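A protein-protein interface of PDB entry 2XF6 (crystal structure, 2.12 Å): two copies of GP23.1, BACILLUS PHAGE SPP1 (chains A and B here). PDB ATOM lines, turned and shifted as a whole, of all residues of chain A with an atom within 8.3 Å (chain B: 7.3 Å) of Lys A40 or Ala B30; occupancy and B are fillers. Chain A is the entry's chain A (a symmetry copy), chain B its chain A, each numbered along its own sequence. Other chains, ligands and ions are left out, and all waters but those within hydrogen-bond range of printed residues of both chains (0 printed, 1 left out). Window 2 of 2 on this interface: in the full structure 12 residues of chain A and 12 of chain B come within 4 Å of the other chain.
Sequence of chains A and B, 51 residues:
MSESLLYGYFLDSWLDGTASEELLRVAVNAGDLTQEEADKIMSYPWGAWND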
ATOM      1  N   SER A   2      25.658  11.685  -6.482  1.00  0.00           N
ATOM      2  CA  SER A   2      25.197  12.484  -7.651  1.00  0.00           C
ATOM      3  C   SER A   2      25.992  12.089  -8.883  1.00  0.00           C
ATOM      4  O   SER A   2      27.092  11.539  -8.777  1.00  0.00           O
ATOM      5  CB  SER A   2      25.325  13.985  -7.375  1.00  0.00           C
ATOM      6  OG  SER A   2      26.651  14.331  -7.020  1.00  0.00           O
ATOM      7  N   GLU A   3      25.430  12.383 -10.049  1.00  0.00           N
ATOM      8  CA  GLU A   3      25.964  11.884 -11.307  1.00  0.00           C
ATOM      9  C   GLU A   3      27.177  12.652 -11.823  1.00  0.00           C
ATOM     10  O   GLU A   3      27.441  13.785 -11.404  1.00  0.00           O
ATOM     11  CB  GLU A   3      24.858  11.841 -12.368  1.00  0.00           C
ATOM     12  CG  GLU A   3      24.075  13.139 -12.528  1.00  0.00           C
ATOM     13  CD  GLU A   3      22.715  12.930 -13.171  1.00  0.00           C
ATOM     14  OE1 GLU A   3      22.350  11.765 -13.463  1.00  0.00           O
ATOM     15  OE2 GLU A   3      22.002  13.939 -13.377  1.00  0.00           O
ATOM     16  N   SER A   4      27.910  12.009 -12.729  1.00  0.00           N
ATOM     17  CA  SER A   4      29.016  12.634 -13.441  1.00  0.00           C
ATOM     18  C   SER A   4      28.493  13.810 -14.255  1.00  0.00           C
ATOM     19  O   SER A   4      27.360  13.781 -14.744  1.00  0.00           O
ATOM     20  CB  SER A   4      29.694  11.618 -14.362  1.00  0.00           C
ATOM     21  OG  SER A   4      30.141  10.486 -13.638  1.00  0.00           O
ATOM     22  N   TYR A   7      26.772  13.121 -17.614  1.00  0.00           N
ATOM     23  CA  TYR A   7      25.716  12.103 -17.663  1.00  0.00           C
ATOM     24  C   TYR A   7      24.595  12.487 -18.625  1.00  0.00           C
ATOM     25  O   TYR A   7      24.204  11.687 -19.475  1.00  0.00           O
ATOM     26  CB  TYR A   7      25.142  11.801 -16.272  1.00  0.00           C
ATOM     27  CG  TYR A   7      24.037  10.762 -16.297  1.00  0.00           C
ATOM     28  CD1 TYR A   7      24.334   9.400 -16.266  1.00  0.00           C
ATOM     29  CD2 TYR A   7      22.696  11.142 -16.369  1.00  0.00           C
ATOM     30  CE1 TYR A   7      23.324   8.442 -16.295  1.00  0.00           C
ATOM     31  CE2 TYR A   7      21.679  10.193 -16.399  1.00  0.00           C
ATOM     32  CZ  TYR A   7      22.001   8.847 -16.363  1.00  0.00           C
ATOM     33  OH  TYR A   7      20.996   7.907 -16.392  1.00  0.00           O
ATOM     34  N   LEU A  11      23.678  10.647 -22.082  1.00  0.00           N
ATOM     35  CA  LEU A  11      22.313  10.127 -22.140  1.00  0.00           C
ATOM     36  C   LEU A  11      21.587  10.661 -23.374  1.00  0.00           C
ATOM     37  O   LEU A  11      20.837   9.931 -24.025  1.00  0.00           O
ATOM     38  CB  LEU A  11      21.538  10.478 -20.863  1.00  0.00           C
ATOM     39  CG  LEU A  11      20.061  10.075 -20.746  1.00  0.00           C
ATOM     40  CD1 LEU A  11      19.874   8.575 -20.927  1.00  0.00           C
ATOM     41  CD2 LEU A  11      19.486  10.529 -19.417  1.00  0.00           C
ATOM     42  N   TRP A  14      22.778   8.917 -26.581  1.00  0.00           N
ATOM     43  CA  TRP A  14      22.191   7.586 -26.694  1.00  0.00           C
ATOM     44  C   TRP A  14      20.755   7.693 -27.197  1.00  0.00           C
ATOM     45  O   TRP A  14      20.322   6.906 -28.041  1.00  0.00           O
ATOM     46  CB  TRP A  14      22.221   6.887 -25.334  1.00  0.00           C
ATOM     47  CG  TRP A  14      21.646   5.497 -25.325  1.00  0.00           C
ATOM     48  CD1 TRP A  14      20.377   5.135 -24.972  1.00  0.00           C
ATOM     49  CD2 TRP A  14      22.327   4.284 -25.670  1.00  0.00           C
ATOM     50  NE1 TRP A  14      20.223   3.774 -25.081  1.00  0.00           N
ATOM     51  CE2 TRP A  14      21.405   3.226 -25.507  1.00  0.00           C
ATOM     52  CE3 TRP A  14      23.626   3.990 -26.104  1.00  0.00           C
ATOM     53  CZ2 TRP A  14      21.740   1.893 -25.763  1.00  0.00           C
ATOM     54  CZ3 TRP A  14      23.960   2.662 -26.359  1.00  0.00           C
ATOM     55  CH2 TRP A  14      23.020   1.632 -26.188  1.00  0.00           C
ATOM     56  N   LEU A  24      30.152   4.605 -24.815  1.00  0.00           N
ATOM     57  CA  LEU A  24      29.805   4.692 -23.398  1.00  0.00           C
ATOM     58  C   LEU A  24      30.851   4.022 -22.512  1.00  0.00           C
ATOM     59  O   LEU A  24      31.115   4.484 -21.402  1.00  0.00           O
ATOM     60  CB  LEU A  24      28.424   4.082 -23.134  1.00  0.00           C
ATOM     61  CG  LEU A  24      27.183   4.790 -23.687  1.00  0.00           C
ATOM     62  CD1 LEU A  24      25.939   3.992 -23.334  1.00  0.00           C
ATOM     63  CD2 LEU A  24      27.060   6.219 -23.164  1.00  0.00           C
ATOM     64  N   LEU A  33      32.025   8.800 -17.009  1.00  0.00           N
ATOM     65  CA  LEU A  33      30.817   8.123 -16.552  1.00  0.00           C
ATOM     66  C   LEU A  33      31.216   6.988 -15.621  1.00  0.00           C
ATOM     67  O   LEU A  33      32.294   6.408 -15.772  1.00  0.00           O
ATOM     68  CB  LEU A  33      30.030   7.543 -17.733  1.00  0.00           C
ATOM     69  CG  LEU A  33      29.288   8.448 -18.721  1.00  0.00           C
ATOM     70  CD1 LEU A  33      28.796   7.627 -19.903  1.00  0.00           C
ATOM     71  CD2 LEU A  33      28.124   9.176 -18.058  1.00  0.00           C
ATOM     72  N   THR A  34      30.357   6.671 -14.656  1.00  0.00           N
ATOM     73  CA  THR A  34      30.543   5.470 -13.850  1.00  0.00           C
ATOM     74  C   THR A  34      29.956   4.286 -14.616  1.00  0.00           C
ATOM     75  O   THR A  34      29.140   4.478 -15.523  1.00  0.00           O
ATOM     76  CB  THR A  34      29.893   5.585 -12.449  1.00  0.00           C
ATOM     77  OG1 THR A  34      28.466   5.636 -12.573  1.00  0.00           O
ATOM     78  CG2 THR A  34      30.390   6.822 -11.708  1.00  0.00           C
ATOM     79  N   GLN A  35      30.380   3.073 -14.266  1.00  0.00           N
ATOM     80  CA  GLN A  35      29.857   1.858 -14.893  1.00  0.00           C
ATOM     81  C   GLN A  35      28.338   1.773 -14.734  1.00  0.00           C
ATOM     82  O   GLN A  35      27.622   1.389 -15.663  1.00  0.00           O
ATOM     83  CB  GLN A  35      30.523   0.611 -14.294  1.00  0.00           C
ATOM     84  CG  GLN A  35      30.036  -0.713 -14.883  1.00  0.00           C
ATOM     85  CD  GLN A  35      30.151  -0.760 -16.396  1.00  0.00           C
ATOM     86  OE1 GLN A  35      31.225  -0.539 -16.954  1.00  0.00           O
ATOM     87  NE2 GLN A  35      29.040  -1.051 -17.067  1.00  0.00           N
ATOM     88  N   GLU A  36      27.874   2.150 -13.546  1.00  0.00           N
ATOM     89  CA  GLU A  36      26.458   2.155 -13.192  1.00  0.00           C
ATOM     90  C   GLU A  36      25.658   3.138 -14.047  1.00  0.00           C
ATOM     91  O   GLU A  36      24.505   2.870 -14.390  1.00  0.00           O
ATOM     92  CB  GLU A  36      26.286   2.493 -11.704  1.00  0.00           C
ATOM     93  CG  GLU A  36      26.983   1.528 -10.733  1.00  0.00           C
ATOM     94  CD  GLU A  36      28.452   1.861 -10.471  1.00  0.00           C
ATOM     95  OE1 GLU A  36      29.010   2.757 -11.140  1.00  0.00           O
ATOM     96  OE2 GLU A  36      29.052   1.217  -9.586  1.00  0.00           O
ATOM     97  N   GLU A  37      26.279   4.269 -14.384  1.00  0.00           N
ATOM     98  CA  GLU A  37      25.659   5.282 -15.238  1.00  0.00           C
ATOM     99  C   GLU A  37      25.497   4.799 -16.675  1.00  0.00           C
ATOM    100  O   GLU A  37      24.481   5.074 -17.314  1.00  0.00           O
ATOM    101  CB  GLU A  37      26.467   6.579 -15.211  1.00  0.00           C
ATOM    102  CG  GLU A  37      26.286   7.398 -13.946  1.00  0.00           C
ATOM    103  CD  GLU A  37      27.246   8.567 -13.860  1.00  0.00           C
ATOM    104  OE1 GLU A  37      28.414   8.430 -14.276  1.00  0.00           O
ATOM    105  OE2 GLU A  37      26.832   9.629 -13.364  1.00  0.00           O
ATOM    106  N   ALA A  38      26.505   4.082 -17.172  1.00  0.00           N
ATOM    107  CA  ALA A  38      26.471   3.512 -18.519  1.00  0.00           C
ATOM    108  C   ALA A  38      25.367   2.469 -18.651  1.00  0.00           C
ATOM    109  O   ALA A  38      24.642   2.449 -19.648  1.00  0.00           O
ATOM    110  CB  ALA A  38      27.818   2.908 -18.876  1.00  0.00           C
ATOM    111  N   ASP A  39      25.234   1.652 -17.625  1.00  0.00           N
ATOM    112  CA  ASP A  39      24.253   0.627 -17.587  1.00  0.00           C
ATOM    113  C   ASP A  39      22.840   1.243 -17.475  1.00  0.00           C
ATOM    114  O   ASP A  39      21.922   0.724 -17.973  1.00  0.00           O
ATOM    115  CB  ASP A  39      24.554  -0.372 -16.472  1.00  0.00           C
ATOM    116  CG  ASP A  39      25.727  -1.309 -16.794  1.00  0.00           C
ATOM    117  OD1 ASP A  39      25.942  -1.760 -17.918  1.00  0.00           O
ATOM    118  OD2 ASP A  39      26.444  -1.615 -15.877  1.00  0.00           O
ATOM    119  N   LYS A  40      22.719   2.365 -16.805  1.00  0.00           N
ATOM    120  CA  LYS A  40      21.512   3.095 -16.723  1.00  0.00           C
ATOM    121  C   LYS A  40      21.093   3.721 -18.047  1.00  0.00           C
ATOM    122  O   LYS A  40      19.965   3.665 -18.403  1.00  0.00           O
ATOM    123  CB  LYS A  40      21.645   4.151 -15.676  1.00  0.00           C
ATOM    124  CG  LYS A  40      20.498   4.971 -15.526  1.00  0.00           C
ATOM    125  CD  LYS A  40      20.324   5.220 -14.132  1.00  0.00           C
ATOM    126  CE  LYS A  40      21.518   5.861 -13.573  1.00  0.00           C
ATOM    127  NZ  LYS A  40      21.391   7.275 -13.678  1.00  0.00           N
ATOM    128  N   ILE A  41      22.038   4.327 -18.748  1.00  0.00           N
ATOM    129  CA  ILE A  41      21.803   4.937 -20.059  1.00  0.00           C
ATOM    130  C   ILE A  41      21.348   3.885 -21.080  1.00  0.00           C
ATOM    131  O   ILE A  41      20.477   4.151 -21.911  1.00  0.00           O
ATOM    132  CB  ILE A  41      23.069   5.696 -20.556  1.00  0.00           C
ATOM    133  CG1 ILE A  41      23.308   6.948 -19.704  1.00  0.00           C
ATOM    134  CG2 ILE A  41      22.943   6.086 -22.021  1.00  0.00           C
ATOM    135  CD1 ILE A  41      24.729   7.493 -19.767  1.00  0.00           C
ATOM    136  N   MET A  42      21.932   2.691 -20.991  1.00  0.00           N
ATOM    137  CA  MET A  42      21.602   1.578 -21.890  1.00  0.00           C
ATOM    138  C   MET A  42      20.236   0.933 -21.613  1.00  0.00           C
ATOM    139  O   MET A  42      19.745   0.141 -22.426  1.00  0.00           O
ATOM    140  CB  MET A  42      22.711   0.524 -21.870  1.00  0.00           C
ATOM    141  CG  MET A  42      23.970   0.931 -22.620  1.00  0.00           C
ATOM    142  SD  MET A  42      25.219  -0.371 -22.689  1.00  0.00           S
ATOM    143  CE  MET A  42      25.903  -0.302 -21.032  1.00  0.00           C
ATOM    144  N   SER A  43      19.674   1.259 -20.488  1.00  0.00           N
ATOM    145  CA  SER A  43      18.354   0.852 -20.147  1.00  0.00           C
ATOM    146  C   SER A  43      17.266   1.681 -20.913  1.00  0.00           C
ATOM    147  O   SER A  43      16.169   1.311 -21.015  1.00  0.00           O
ATOM    148  CB  SER A  43      18.240   0.779 -18.638  1.00  0.00           C
ATOM    149  OG  SER A  43      17.535   1.847 -18.172  1.00  0.00           O
ATOM    150  N   TYR A  44      17.665   2.775 -21.503  1.00  0.00           N
ATOM    151  CA  TYR A  44      16.777   3.586 -22.330  1.00  0.00           C
ATOM    152  C   TYR A  44      16.719   3.037 -23.751  1.00  0.00           C
ATOM    153  O   TYR A  44      17.669   2.393 -24.207  1.00  0.00           O
ATOM    154  CB  TYR A  44      17.355   5.004 -22.391  1.00  0.00           C
ATOM    155  CG  TYR A  44      17.122   5.837 -21.157  1.00  0.00           C
ATOM    156  CD1 TYR A  44      16.088   6.770 -21.112  1.00  0.00           C
ATOM    157  CD2 TYR A  44      17.941   5.703 -20.038  1.00  0.00           C
ATOM    158  CE1 TYR A  44      15.870   7.545 -19.980  1.00  0.00           C
ATOM    159  CE2 TYR A  44      17.732   6.472 -18.900  1.00  0.00           C
ATOM    160  CZ  TYR A  44      16.696   7.390 -18.879  1.00  0.00           C
ATOM    161  OH  TYR A  44      16.492   8.152 -17.754  1.00  0.00           O
ATOM    162  N   PRO A  45      15.600   3.289 -24.454  1.00  0.00           N
ATOM    163  CA  PRO A  45      15.516   2.945 -25.866  1.00  0.00           C
ATOM    164  C   PRO A  45      16.505   3.777 -26.666  1.00  0.00           C
ATOM    165  O   PRO A  45      16.408   5.007 -26.705  1.00  0.00           O
ATOM    166  CB  PRO A  45      14.073   3.313 -26.238  1.00  0.00           C
ATOM    167  CG  PRO A  45      13.337   3.359 -24.945  1.00  0.00           C
ATOM    168  CD  PRO A  45      14.335   3.859 -23.957  1.00  0.00           C
ATOM    169  N   LEU B   6      17.693  16.573 -14.682  1.00  0.00           N
ATOM    170  CA  LEU B   6      17.215  16.402 -16.051  1.00  0.00           C
ATOM    171  C   LEU B   6      15.720  16.697 -16.235  1.00  0.00           C
ATOM    172  O   LEU B   6      15.135  16.312 -17.250  1.00  0.00           O
ATOM    173  CB  LEU B   6      17.561  14.995 -16.561  1.00  0.00           C
ATOM    174  CG  LEU B   6      19.049  14.638 -16.661  1.00  0.00           C
ATOM    175  CD1 LEU B   6      19.238  13.130 -16.709  1.00  0.00           C
ATOM    176  CD2 LEU B   6      19.713  15.310 -17.863  1.00  0.00           C
ATOM    177  N   PHE B  10      13.819  16.604 -19.878  1.00  0.00           N
ATOM    178  CA  PHE B  10      12.709  15.697 -20.171  1.00  0.00           C
ATOM    179  C   PHE B  10      11.386  16.427 -20.407  1.00  0.00           C
ATOM    180  O   PHE B  10      10.509  15.917 -21.109  1.00  0.00           O
ATOM    181  CB  PHE B  10      12.554  14.635 -19.076  1.00  0.00           C
ATOM    182  CG  PHE B  10      13.588  13.541 -19.137  1.00  0.00           C
ATOM    183  CD1 PHE B  10      13.632  12.663 -20.218  1.00  0.00           C
ATOM    184  CD2 PHE B  10      14.511  13.380 -18.108  1.00  0.00           C
ATOM    185  CE1 PHE B  10      14.587  11.651 -20.275  1.00  0.00           C
ATOM    186  CE2 PHE B  10      15.467  12.368 -18.157  1.00  0.00           C
ATOM    187  CZ  PHE B  10      15.504  11.502 -19.242  1.00  0.00           C
ATOM    188  N   LEU B  24       9.436   8.537 -20.298  1.00  0.00           N
ATOM    189  CA  LEU B  24       9.370   9.213 -19.004  1.00  0.00           C
ATOM    190  C   LEU B  24       9.378   8.225 -17.842  1.00  0.00           C
ATOM    191  O   LEU B  24       9.943   8.509 -16.786  1.00  0.00           O
ATOM    192  CB  LEU B  24       8.133  10.113 -18.920  1.00  0.00           C
ATOM    193  CG  LEU B  24       8.065  11.364 -19.803  1.00  0.00           C
ATOM    194  CD1 LEU B  24       6.744  12.078 -19.577  1.00  0.00           C
ATOM    195  CD2 LEU B  24       9.231  12.314 -19.538  1.00  0.00           C
ATOM    196  N   ARG B  25       8.755   7.067 -18.051  1.00  0.00           N
ATOM    197  CA  ARG B  25       8.689   6.025 -17.030  1.00  0.00           C
ATOM    198  C   ARG B  25      10.012   5.273 -16.890  1.00  0.00           C
ATOM    199  O   ARG B  25      10.371   4.852 -15.789  1.00  0.00           O
ATOM    200  CB  ARG B  25       7.527   5.069 -17.307  1.00  0.00           C
ATOM    201  CG  ARG B  25       6.162   5.740 -17.228  1.00  0.00           C
ATOM    202  CD  ARG B  25       5.031   4.748 -17.397  1.00  0.00           C
ATOM    203  NE  ARG B  25       3.722   5.400 -17.385  1.00  0.00           N
ATOM    204  CZ  ARG B  25       2.994   5.622 -16.293  1.00  0.00           C
ATOM    205  NH1 ARG B  25       3.433   5.244 -15.099  1.00  0.00           N
ATOM    206  NH2 ARG B  25       1.817   6.224 -16.396  1.00  0.00           N
ATOM    207  N   VAL B  26      10.727   5.115 -18.005  1.00  0.00           N
ATOM    208  CA  VAL B  26      12.092   4.580 -18.005  1.00  0.00           C
ATOM    209  C   VAL B  26      12.996   5.492 -17.172  1.00  0.00           C
ATOM    210  O   VAL B  26      13.859   5.023 -16.428  1.00  0.00           O
ATOM    211  CB  VAL B  26      12.665   4.468 -19.445  1.00  0.00           C
ATOM    212  CG1 VAL B  26      14.124   4.034 -19.419  1.00  0.00           C
ATOM    213  CG2 VAL B  26      11.839   3.497 -20.278  1.00  0.00           C
ATOM    214  N   ALA B  27      12.776   6.798 -17.311  1.00  0.00           N
ATOM    215  CA  ALA B  27      13.509   7.810 -16.556  1.00  0.00           C
ATOM    216  C   ALA B  27      13.139   7.801 -15.075  1.00  0.00           C
ATOM    217  O   ALA B  27      13.981   8.086 -14.220  1.00  0.00           O
ATOM    218  CB  ALA B  27      13.282   9.189 -17.156  1.00  0.00           C
ATOM    219  N   VAL B  28      11.877   7.481 -14.782  1.00  0.00           N
ATOM    220  CA  VAL B  28      11.420   7.302 -13.402  1.00  0.00           C
ATOM    221  C   VAL B  28      12.118   6.098 -12.769  1.00  0.00           C
ATOM    222  O   VAL B  28      12.653   6.206 -11.659  1.00  0.00           O
ATOM    223  CB  VAL B  28       9.873   7.183 -13.295  1.00  0.00           C
ATOM    224  CG1 VAL B  28       9.446   6.739 -11.895  1.00  0.00           C
ATOM    225  CG2 VAL B  28       9.217   8.505 -13.638  1.00  0.00           C
ATOM    226  N   ASN B  29      12.141   4.992 -13.454  1.00  0.00           N
ATOM    227  CA  ASN B  29      12.807   3.877 -12.864  1.00  0.00           C
ATOM    228  C   ASN B  29      14.312   3.983 -12.855  1.00  0.00           C
ATOM    229  O   ASN B  29      14.909   3.437 -11.984  1.00  0.00           O
ATOM    230  CB  ASN B  29      12.218   2.561 -13.272  1.00  0.00           C
ATOM    231  CG  ASN B  29      10.898   2.297 -12.513  1.00  0.00           C
ATOM    232  OD1 ASN B  29      10.859   1.644 -11.484  1.00  0.00           O
ATOM    233  ND2 ASN B  29       9.831   2.874 -13.012  1.00  0.00           N
ATOM    234  N   ALA B  30      14.871   4.798 -13.763  1.00  0.00           N
ATOM    235  CA  ALA B  30      16.309   5.087 -13.763  1.00  0.00           C
ATOM    236  C   ALA B  30      16.698   5.988 -12.595  1.00  0.00           C
ATOM    237  O   ALA B  30      17.836   5.957 -12.128  1.00  0.00           O
ATOM    238  CB  ALA B  30      16.724   5.724 -15.083  1.00  0.00           C
ATOM    239  N   GLY B  31      15.740   6.781 -12.124  1.00  0.00           N
ATOM    240  CA  GLY B  31      15.982   7.725 -11.039  1.00  0.00           C
ATOM    241  C   GLY B  31      16.431   9.081 -11.550  1.00  0.00           C
ATOM    242  O   GLY B  31      16.935   9.904 -10.784  1.00  0.00           O
ATOM    243  N   ASP B  32      16.248   9.305 -12.850  1.00  0.00           N
ATOM    244  CA  ASP B  32      16.562  10.589 -13.477  1.00  0.00           C
ATOM    245  C   ASP B  32      15.378  11.550 -13.383  1.00  0.00           C
ATOM    246  O   ASP B  32      15.511  12.747 -13.648  1.00  0.00           O
ATOM    247  CB  ASP B  32      16.988  10.385 -14.936  1.00  0.00           C
ATOM    248  CG  ASP B  32      18.297   9.618 -15.065  1.00  0.00           C
ATOM    249  OD1 ASP B  32      19.175   9.762 -14.186  1.00  0.00           O
ATOM    250  OD2 ASP B  32      18.452   8.874 -16.055  1.00  0.00           O
ATOM    251  N   LEU B  33      14.221  11.002 -13.013  1.00  0.00           N
ATOM    252  CA  LEU B  33      13.024  11.774 -12.699  1.00  0.00           C
ATOM    253  C   LEU B  33      12.297  11.097 -11.546  1.00  0.00           C
ATOM    254  O   LEU B  33      12.367   9.875 -11.397  1.00  0.00           O
ATOM    255  CB  LEU B  33      12.082  11.845 -13.906  1.00  0.00           C
ATOM    256  CG  LEU B  33      12.430  12.675 -15.145  1.00  0.00           C
ATOM    257  CD1 LEU B  33      11.439  12.380 -16.259  1.00  0.00           C
ATOM    258  CD2 LEU B  33      12.457  14.168 -14.837  1.00  0.00           C
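Positions printed for both chains: 24 and 33.
OD1 of Asp B32 touches OE1 of Glu A3, 3.8 Å away. Tyr A7 touches Leu B6 (CE2 to CD1, 3.8 Å). Leu A11 touches Leu B6 (CD2 to CD1, 3.8 Å). Asp B32 touches Leu A11. Ala B30 touches Lys A40. Val B26 touches Ser A43 (CG1 to O, 3.8 Å). Tyr A44 touches Phe B10 (OH to CZ, 3.8 Å). Val B26 touches Tyr A44. CA of Ala B27 touches OH of Tyr A44, at 3.2 Å. Tyr A44 touches Ala B30.
O of Ala B27 sits at hydrogen-bond distance from N of Asp B32 (2.9 Å). The backbone carbonyl oxygen (O) of Ala B27 is in hydrogen-bond range of the backbone NH (N) of Leu B33 (3.2 Å). The side-chain hydroxyl of Tyr A7 is in hydrogen-bond range of the side-chain amino group of Lys A40, at 2.8 Å. NE1 of Trp A14 is in hydrogen-bond range of O of Tyr A44 (3.0 Å). The backbone carbonyl oxygen (O) of Lys A40 sits at hydrogen-bond distance from the side-chain hydroxyl (OG) of Ser A43, at 3.0 Å.
The side-chain carboxylate (OD2) of Asp B32 is in hydrogen-bond range of the side-chain hydroxyl (OH) of Tyr A7 (2.7 Å). The side-chain amino group (NZ) of Lys A40 lies within salt-bridge range of the side-chain carboxylate (OD1) of Asp B32. The side-chain hydroxyl of Tyr A44 sits at hydrogen-bond distance from the side-chain carboxylate of Asp B32 (2.7 Å).
Printed residues of chain B that touch a printed residue of chain A: Leu B6, Phe B10, Val B26, Ala B27, Ala B30 and Asp B32. Hydrophobic or aromatic side chains of chain B within 4 Å of the printed part of chain A: Leu B6, Phe B10, Val B26, Ala B27 and Ala B30. Of the 20 printed residues of chain A, 6 touch a printed residue of chain B. Hydrophobic or aromatic side chains of chain A within 4 Å of the printed part of chain B: Tyr A7, Leu A11 and Tyr A44. Among the printed residues, 13 pairs touch across the chains. Among the printed residues, Asp or Glu carboxylates within 4 Å of a Lys or Arg side-chain nitrogen of the other chain: Lys A40 with Asp B32 (3.4 Å).
Lys A40 touches two residues of chain B. Ala B30 touches just these residues of chain A: Lys A40 (3.3 Å) and Tyr A44 (3.6 Å). Printed residues of chain B within 4 Å of Leu A11: Leu B6 (3.8 Å) and Asp B32 (3.9 Å). Of the printed residues of chain A, Ala B27 touches Tyr A44 (3.2 Å). Printed residues of chain B within 4 Å of Glu A3: Asp B32 (3.8 Å). Printed residues of chain A within 4 Å of Asp B32: Glu A3 (3.8 Å), Tyr A7 (2.7 Å), Leu A11 (3.9 Å), Lys A40 (3.4 Å) and Tyr A44 (2.7 Å). Of the printed residues of chain A, Leu B6 touches Tyr A7 (3.8 Å) and Leu A11 (3.8 Å). Leu A24 touches none of the printed residues of chain B. Ile A41 touches none of the printed residues of chain B. The nearest residue of chain B that does not touch Lys A40 is Gly B31 (5.2 Å).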
